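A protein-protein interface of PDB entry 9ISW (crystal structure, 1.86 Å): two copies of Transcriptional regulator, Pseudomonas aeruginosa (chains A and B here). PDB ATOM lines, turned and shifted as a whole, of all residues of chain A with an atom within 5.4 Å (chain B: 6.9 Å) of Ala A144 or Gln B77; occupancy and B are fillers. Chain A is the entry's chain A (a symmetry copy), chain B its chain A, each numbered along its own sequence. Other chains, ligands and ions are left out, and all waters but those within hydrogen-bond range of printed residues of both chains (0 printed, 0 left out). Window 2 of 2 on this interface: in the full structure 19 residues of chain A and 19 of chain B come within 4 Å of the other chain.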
ATOM      1  N   LEU A  93     -19.806  -3.863  11.490  1.00  0.00           N
ATOM      2  CA  LEU A  93     -21.251  -3.892  11.268  1.00  0.00           C
ATOM      3  C   LEU A  93     -21.907  -5.007  12.074  1.00  0.00           C
ATOM      4  O   LEU A  93     -22.910  -4.788  12.772  1.00  0.00           O
ATOM      5  CB  LEU A  93     -21.542  -4.092   9.775  1.00  0.00           C
ATOM      6  CG  LEU A  93     -21.731  -2.891   8.849  1.00  0.00           C
ATOM      7  CD1 LEU A  93     -22.134  -3.375   7.455  1.00  0.00           C
ATOM      8  CD2 LEU A  93     -22.757  -1.891   9.411  1.00  0.00           C
ATOM      9  N   SER A  96     -22.026  -4.441  15.763  1.00  0.00           N
ATOM     10  CA  SER A  96     -23.065  -3.482  16.136  1.00  0.00           C
ATOM     11  C   SER A  96     -24.453  -4.117  16.134  1.00  0.00           C
ATOM     12  O   SER A  96     -25.282  -3.802  16.990  1.00  0.00           O
ATOM     13  CB  SER A  96     -23.050  -2.272  15.208  1.00  0.00           C
ATOM     14  OG  SER A  96     -22.258  -1.237  15.755  1.00  0.00           O
ATOM     15  N   ARG A 100     -26.761  -4.411  19.535  1.00  0.00           N
ATOM     16  CA  ARG A 100     -27.873  -3.478  19.569  1.00  0.00           C
ATOM     17  C   ARG A 100     -29.245  -4.103  19.358  1.00  0.00           C
ATOM     18  O   ARG A 100     -30.239  -3.473  19.738  1.00  0.00           O
ATOM     19  CB  ARG A 100     -27.663  -2.373  18.538  1.00  0.00           C
ATOM     20  CG  ARG A 100     -26.388  -1.589  18.813  1.00  0.00           C
ATOM     21  CD  ARG A 100     -26.644  -0.114  18.966  1.00  0.00           C
ATOM     22  NE  ARG A 100     -25.439   0.553  19.442  1.00  0.00           N
ATOM     23  CZ  ARG A 100     -24.625   1.267  18.675  1.00  0.00           C
ATOM     24  NH1 ARG A 100     -24.902   1.438  17.382  1.00  0.00           N
ATOM     25  NH2 ARG A 100     -23.544   1.824  19.209  1.00  0.00           N
ATOM     26  N   ALA A 140     -28.000  -4.219   8.049  1.00  0.00           N
ATOM     27  CA  ALA A 140     -27.241  -3.984   9.269  1.00  0.00           C
ATOM     28  C   ALA A 140     -27.105  -2.497   9.597  1.00  0.00           C
ATOM     29  O   ALA A 140     -26.916  -2.144  10.768  1.00  0.00           O
ATOM     30  CB  ALA A 140     -25.856  -4.629   9.148  1.00  0.00           C
ATOM     31  N   PHE A 141     -27.190  -1.620   8.593  1.00  0.00           N
ATOM     32  CA  PHE A 141     -26.936  -0.191   8.817  1.00  0.00           C
ATOM     33  C   PHE A 141     -27.765   0.423   9.938  1.00  0.00           C
ATOM     34  O   PHE A 141     -27.195   1.202  10.734  1.00  0.00           O
ATOM     35  CB  PHE A 141     -27.153   0.586   7.510  1.00  0.00           C
ATOM     36  CG  PHE A 141     -26.123   0.289   6.443  1.00  0.00           C
ATOM     37  CD1 PHE A 141     -24.842  -0.113   6.785  1.00  0.00           C
ATOM     38  CD2 PHE A 141     -26.445   0.411   5.097  1.00  0.00           C
ATOM     39  CE1 PHE A 141     -23.885  -0.380   5.802  1.00  0.00           C
ATOM     40  CE2 PHE A 141     -25.498   0.138   4.107  1.00  0.00           C
ATOM     41  CZ  PHE A 141     -24.219  -0.258   4.464  1.00  0.00           C
ATOM     42  N   PRO A 142     -29.070   0.186  10.058  1.00  0.00           N
ATOM     43  CA  PRO A 142     -29.838   0.833  11.142  1.00  0.00           C
ATOM     44  C   PRO A 142     -29.366   0.479  12.541  1.00  0.00           C
ATOM     45  O   PRO A 142     -29.625   1.249  13.479  1.00  0.00           O
ATOM     46  CB  PRO A 142     -31.273   0.342  10.912  1.00  0.00           C
ATOM     47  CG  PRO A 142     -31.328  -0.044   9.467  1.00  0.00           C
ATOM     48  CD  PRO A 142     -29.953  -0.557   9.129  1.00  0.00           C
ATOM     49  N   PHE A 143     -28.715  -0.674  12.731  1.00  0.00           N
ATOM     50  CA  PHE A 143     -28.237  -1.033  14.059  1.00  0.00           C
ATOM     51  C   PHE A 143     -26.996  -0.236  14.417  1.00  0.00           C
ATOM     52  O   PHE A 143     -26.818   0.158  15.570  1.00  0.00           O
ATOM     53  CB  PHE A 143     -27.912  -2.525  14.135  1.00  0.00           C
ATOM     54  CG  PHE A 143     -29.105  -3.420  13.934  1.00  0.00           C
ATOM     55  CD1 PHE A 143     -29.491  -3.803  12.659  1.00  0.00           C
ATOM     56  CD2 PHE A 143     -29.828  -3.888  15.025  1.00  0.00           C
ATOM     57  CE1 PHE A 143     -30.590  -4.639  12.473  1.00  0.00           C
ATOM     58  CE2 PHE A 143     -30.931  -4.718  14.855  1.00  0.00           C
ATOM     59  CZ  PHE A 143     -31.311  -5.101  13.581  1.00  0.00           C
ATOM     60  N   ALA A 144     -26.127  -0.017  13.427  1.00  0.00           N
ATOM     61  CA  ALA A 144     -24.868   0.691  13.641  1.00  0.00           C
ATOM     62  C   ALA A 144     -25.085   2.192  13.772  1.00  0.00           C
ATOM     63  O   ALA A 144     -24.377   2.861  14.539  1.00  0.00           O
ATOM     64  CB  ALA A 144     -23.906   0.403  12.482  1.00  0.00           C
ATOM     65  N   ASN A 145     -26.040   2.740  13.017  1.00  0.00           N
ATOM     66  CA  ASN A 145     -26.253   4.193  12.921  1.00  0.00           C
ATOM     67  C   ASN A 145     -24.924   4.929  12.804  1.00  0.00           C
ATOM     68  O   ASN A 145     -24.639   5.896  13.520  1.00  0.00           O
ATOM     69  CB  ASN A 145     -27.058   4.722  14.109  1.00  0.00           C
ATOM     70  CG  ASN A 145     -27.574   6.108  13.872  1.00  0.00           C
ATOM     71  OD1 ASN A 145     -27.703   6.540  12.720  1.00  0.00           O
ATOM     72  ND2 ASN A 145     -27.835   6.842  14.953  1.00  0.00           N
ATOM     73  N   ASN A 146     -24.090   4.438  11.890  1.00  0.00           N
ATOM     74  CA  ASN A 146     -22.714   4.900  11.735  1.00  0.00           C
ATOM     75  C   ASN A 146     -22.565   5.435  10.317  1.00  0.00           C
ATOM     76  O   ASN A 146     -22.347   4.654   9.376  1.00  0.00           O
ATOM     77  CB  ASN A 146     -21.737   3.753  12.007  1.00  0.00           C
ATOM     78  CG  ASN A 146     -20.300   4.181  11.945  1.00  0.00           C
ATOM     79  OD1 ASN A 146     -19.950   5.096  11.209  1.00  0.00           O
ATOM     80  ND2 ASN A 146     -19.436   3.495  12.710  1.00  0.00           N
ATOM     81  N   LEU A 149     -19.129   4.507   8.526  1.00  0.00           N
ATOM     82  CA  LEU A 149     -19.073   3.100   8.155  1.00  0.00           C
ATOM     83  C   LEU A 149     -20.029   2.791   7.012  1.00  0.00           C
ATOM     84  O   LEU A 149     -19.667   2.087   6.066  1.00  0.00           O
ATOM     85  CB  LEU A 149     -19.406   2.254   9.389  1.00  0.00           C
ATOM     86  CG  LEU A 149     -19.519   0.743   9.229  1.00  0.00           C
ATOM     87  CD1 LEU A 149     -18.190   0.189   8.766  1.00  0.00           C
ATOM     88  CD2 LEU A 149     -19.917   0.146  10.571  1.00  0.00           C
ATOM     89  N   LEU B  74     -21.735  18.210  15.442  1.00  0.00           N
ATOM     90  CA  LEU B  74     -21.091  17.059  16.054  1.00  0.00           C
ATOM     91  C   LEU B  74     -22.060  16.409  17.022  1.00  0.00           C
ATOM     92  O   LEU B  74     -22.878  17.083  17.641  1.00  0.00           O
ATOM     93  CB  LEU B  74     -19.814  17.444  16.806  1.00  0.00           C
ATOM     94  CG  LEU B  74     -18.794  18.251  15.984  1.00  0.00           C
ATOM     95  CD1 LEU B  74     -17.701  18.849  16.860  1.00  0.00           C
ATOM     96  CD2 LEU B  74     -18.204  17.347  14.916  1.00  0.00           C
ATOM     97  N   SER B  75     -21.968  15.093  17.140  1.00  0.00           N
ATOM     98  CA  SER B  75     -22.751  14.381  18.130  1.00  0.00           C
ATOM     99  C   SER B  75     -21.909  13.250  18.718  1.00  0.00           C
ATOM    100  O   SER B  75     -20.995  12.740  18.059  1.00  0.00           O
ATOM    101  CB  SER B  75     -24.040  13.802  17.530  1.00  0.00           C
ATOM    102  OG  SER B  75     -23.721  12.762  16.637  1.00  0.00           O
ATOM    103  N   PRO B  76     -22.210  12.853  19.958  1.00  0.00           N
ATOM    104  CA  PRO B  76     -21.452  11.738  20.559  1.00  0.00           C
ATOM    105  C   PRO B  76     -21.506  10.471  19.728  1.00  0.00           C
ATOM    106  O   PRO B  76     -20.476   9.812  19.559  1.00  0.00           O
ATOM    107  CB  PRO B  76     -22.128  11.557  21.930  1.00  0.00           C
ATOM    108  CG  PRO B  76     -22.695  12.954  22.243  1.00  0.00           C
ATOM    109  CD  PRO B  76     -23.099  13.536  20.922  1.00  0.00           C
ATOM    110  N   GLN B  77     -22.679  10.112  19.189  1.00  0.00           N
ATOM    111  CA  GLN B  77     -22.765   8.864  18.419  1.00  0.00           C
ATOM    112  C   GLN B  77     -21.940   8.931  17.137  1.00  0.00           C
ATOM    113  O   GLN B  77     -21.335   7.930  16.739  1.00  0.00           O
ATOM    114  CB  GLN B  77     -24.228   8.532  18.109  1.00  0.00           C
ATOM    115  CG  GLN B  77     -24.465   7.477  17.021  1.00  0.00           C
ATOM    116  CD  GLN B  77     -23.768   6.145  17.266  1.00  0.00           C
ATOM    117  OE1 GLN B  77     -23.270   5.857  18.370  1.00  0.00           O
ATOM    118  NE2 GLN B  77     -23.716   5.319  16.220  1.00  0.00           N
ATOM    119  N   HIS B  78     -21.883  10.093  16.482  1.00  0.00           N
ATOM    120  CA  HIS B  78     -21.060  10.191  15.279  1.00  0.00           C
ATOM    121  C   HIS B  78     -19.579  10.218  15.626  1.00  0.00           C
ATOM    122  O   HIS B  78     -18.760   9.629  14.918  1.00  0.00           O
ATOM    123  CB  HIS B  78     -21.441  11.428  14.478  1.00  0.00           C
ATOM    124  CG  HIS B  78     -22.733  11.273  13.742  1.00  0.00           C
ATOM    125  ND1 HIS B  78     -23.321  12.308  13.051  1.00  0.00           N
ATOM    126  CD2 HIS B  78     -23.540  10.196  13.577  1.00  0.00           C
ATOM    127  CE1 HIS B  78     -24.443  11.880  12.499  1.00  0.00           C
ATOM    128  NE2 HIS B  78     -24.604  10.605  12.811  1.00  0.00           N
ATOM    129  N   VAL B  79     -19.211  10.905  16.701  1.00  0.00           N
ATOM    130  CA  VAL B  79     -17.811  10.868  17.126  1.00  0.00           C
ATOM    131  C   VAL B  79     -17.394   9.436  17.450  1.00  0.00           C
ATOM    132  O   VAL B  79     -16.339   8.959  17.014  1.00  0.00           O
ATOM    133  CB  VAL B  79     -17.597  11.801  18.325  1.00  0.00           C
ATOM    134  CG1 VAL B  79     -16.253  11.474  19.016  1.00  0.00           C
ATOM    135  CG2 VAL B  79     -17.657  13.247  17.870  1.00  0.00           C
ATOM    136  N   GLU B  80     -18.207   8.730  18.234  1.00  0.00           N
ATOM    137  CA  GLU B  80     -17.878   7.339  18.551  1.00  0.00           C
ATOM    138  C   GLU B  80     -17.828   6.480  17.292  1.00  0.00           C
ATOM    139  O   GLU B  80     -16.965   5.601  17.158  1.00  0.00           O
ATOM    140  CB  GLU B  80     -18.905   6.786  19.541  1.00  0.00           C
ATOM    141  CG  GLU B  80     -18.789   7.481  20.876  1.00  0.00           C
ATOM    142  CD  GLU B  80     -20.007   7.341  21.752  1.00  0.00           C
ATOM    143  OE1 GLU B  80     -19.976   7.946  22.842  1.00  0.00           O
ATOM    144  OE2 GLU B  80     -20.979   6.653  21.369  1.00  0.00           O
ATOM    145  N   SER B  81     -18.762   6.716  16.370  1.00  0.00           N
ATOM    146  CA  SER B  81     -18.766   6.037  15.070  1.00  0.00           C
ATOM    147  C   SER B  81     -17.453   6.245  14.325  1.00  0.00           C
ATOM    148  O   SER B  81     -16.868   5.302  13.765  1.00  0.00           O
ATOM    149  CB  SER B  81     -19.912   6.588  14.222  1.00  0.00           C
ATOM    150  OG  SER B  81     -21.167   6.081  14.625  1.00  0.00           O
ATOM    151  N   LEU B  82     -17.026   7.504  14.238  1.00  0.00           N
ATOM    152  CA  LEU B  82     -15.812   7.844  13.501  1.00  0.00           C
ATOM    153  C   LEU B  82     -14.594   7.174  14.120  1.00  0.00           C
ATOM    154  O   LEU B  82     -13.762   6.586  13.413  1.00  0.00           O
ATOM    155  CB  LEU B  82     -15.647   9.360  13.484  1.00  0.00           C
ATOM    156  CG  LEU B  82     -14.433   9.914  12.757  1.00  0.00           C
ATOM    157  CD1 LEU B  82     -14.499   9.544  11.280  1.00  0.00           C
ATOM    158  CD2 LEU B  82     -14.417  11.416  12.942  1.00  0.00           C
ATOM    159  N   LEU B 213     -15.378  13.682  23.413  1.00  0.00           N
ATOM    160  CA  LEU B 213     -16.698  13.603  24.041  1.00  0.00           C
ATOM    161  C   LEU B 213     -16.819  14.565  25.215  1.00  0.00           C
ATOM    162  O   LEU B 213     -17.879  15.174  25.424  1.00  0.00           O
ATOM    163  CB  LEU B 213     -16.984  12.167  24.491  1.00  0.00           C
ATOM    164  CG  LEU B 213     -17.135  11.141  23.350  1.00  0.00           C
ATOM    165  CD1 LEU B 213     -17.258   9.702  23.881  1.00  0.00           C
ATOM    166  CD2 LEU B 213     -18.321  11.465  22.437  1.00  0.00           C
ATOM    167  N   LEU B 216     -17.519  17.889  23.694  1.00  0.00           N
ATOM    168  CA  LEU B 216     -18.906  17.934  23.242  1.00  0.00           C
ATOM    169  C   LEU B 216     -19.861  18.170  24.404  1.00  0.00           C
ATOM    170  O   LEU B 216     -20.852  18.898  24.266  1.00  0.00           O
ATOM    171  CB  LEU B 216     -19.281  16.629  22.536  1.00  0.00           C
ATOM    172  CG  LEU B 216     -18.663  16.301  21.173  1.00  0.00           C
ATOM    173  CD1 LEU B 216     -19.572  15.297  20.456  1.00  0.00           C
ATOM    174  CD2 LEU B 216     -18.488  17.565  20.341  1.00  0.00           C
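Asn A145 touches Ser B81.
OG of Ser B81 is in hydrogen-bond range of O of Gln B77 (2.8 Å). The backbone carbonyl oxygen (O) of Ala A144 lies within hydrogen-bond range of the guanidinium group (NH1) of Arg A100, 3.2 Å away. N of Leu A149 lies within hydrogen-bond range of OD1 of Asn A146, 2.9 Å away.
Of the printed residues of chain B, Asn A145 touches Gln B77 (2.9 Å) and Ser B81 (3.6 Å). Printed residues of chain B within 4 Å of Asn A146: Ser B81. Printed residues of chain A within 4 Å of Gln B77: Ala A144 (3.1 Å) and Asn A145 (2.9 Å). Of the printed residues of chain A, Ser B81 touches Asn A145 and Asn A146. The nearest residue of chain B that does not touch Ala A144 is Ser B81 (4.5 Å). The nearest residue of chain A that does not touch Gln B77 is Arg A100 (4.1 Å). The nearest printed residue of chain B that does not touch Asn A145 is His B78 (4.4 Å).
No position is printed for both chains. Of the 4 pairs that touch across the chains among the printed residues, none has its exchanged pair printed and touching as well.
Along chain B the printed residues that touch a printed residue of chain A span positions 77 to 81. Of the 11 printed residues of chain A, 3 touch a printed residue of chain B. Printed residues of chain A that touch a printed residue of chain B: Ala A144, Asn A145 and Asn A146.
NE2 of Gln B77 is in hydrogen-bond range of O of Ala A144 (3.1 Å). The backbone carbonyl oxygen (O) of Asn A145 lies within hydrogen-bond range of the side-chain amide nitrogen (NE2) of Gln B77, 2.9 Å away. The backbone carbonyl oxygen (O) of Ser B81 sits at hydrogen-bond distance from the side-chain amide nitrogen (ND2) of Asn A146.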
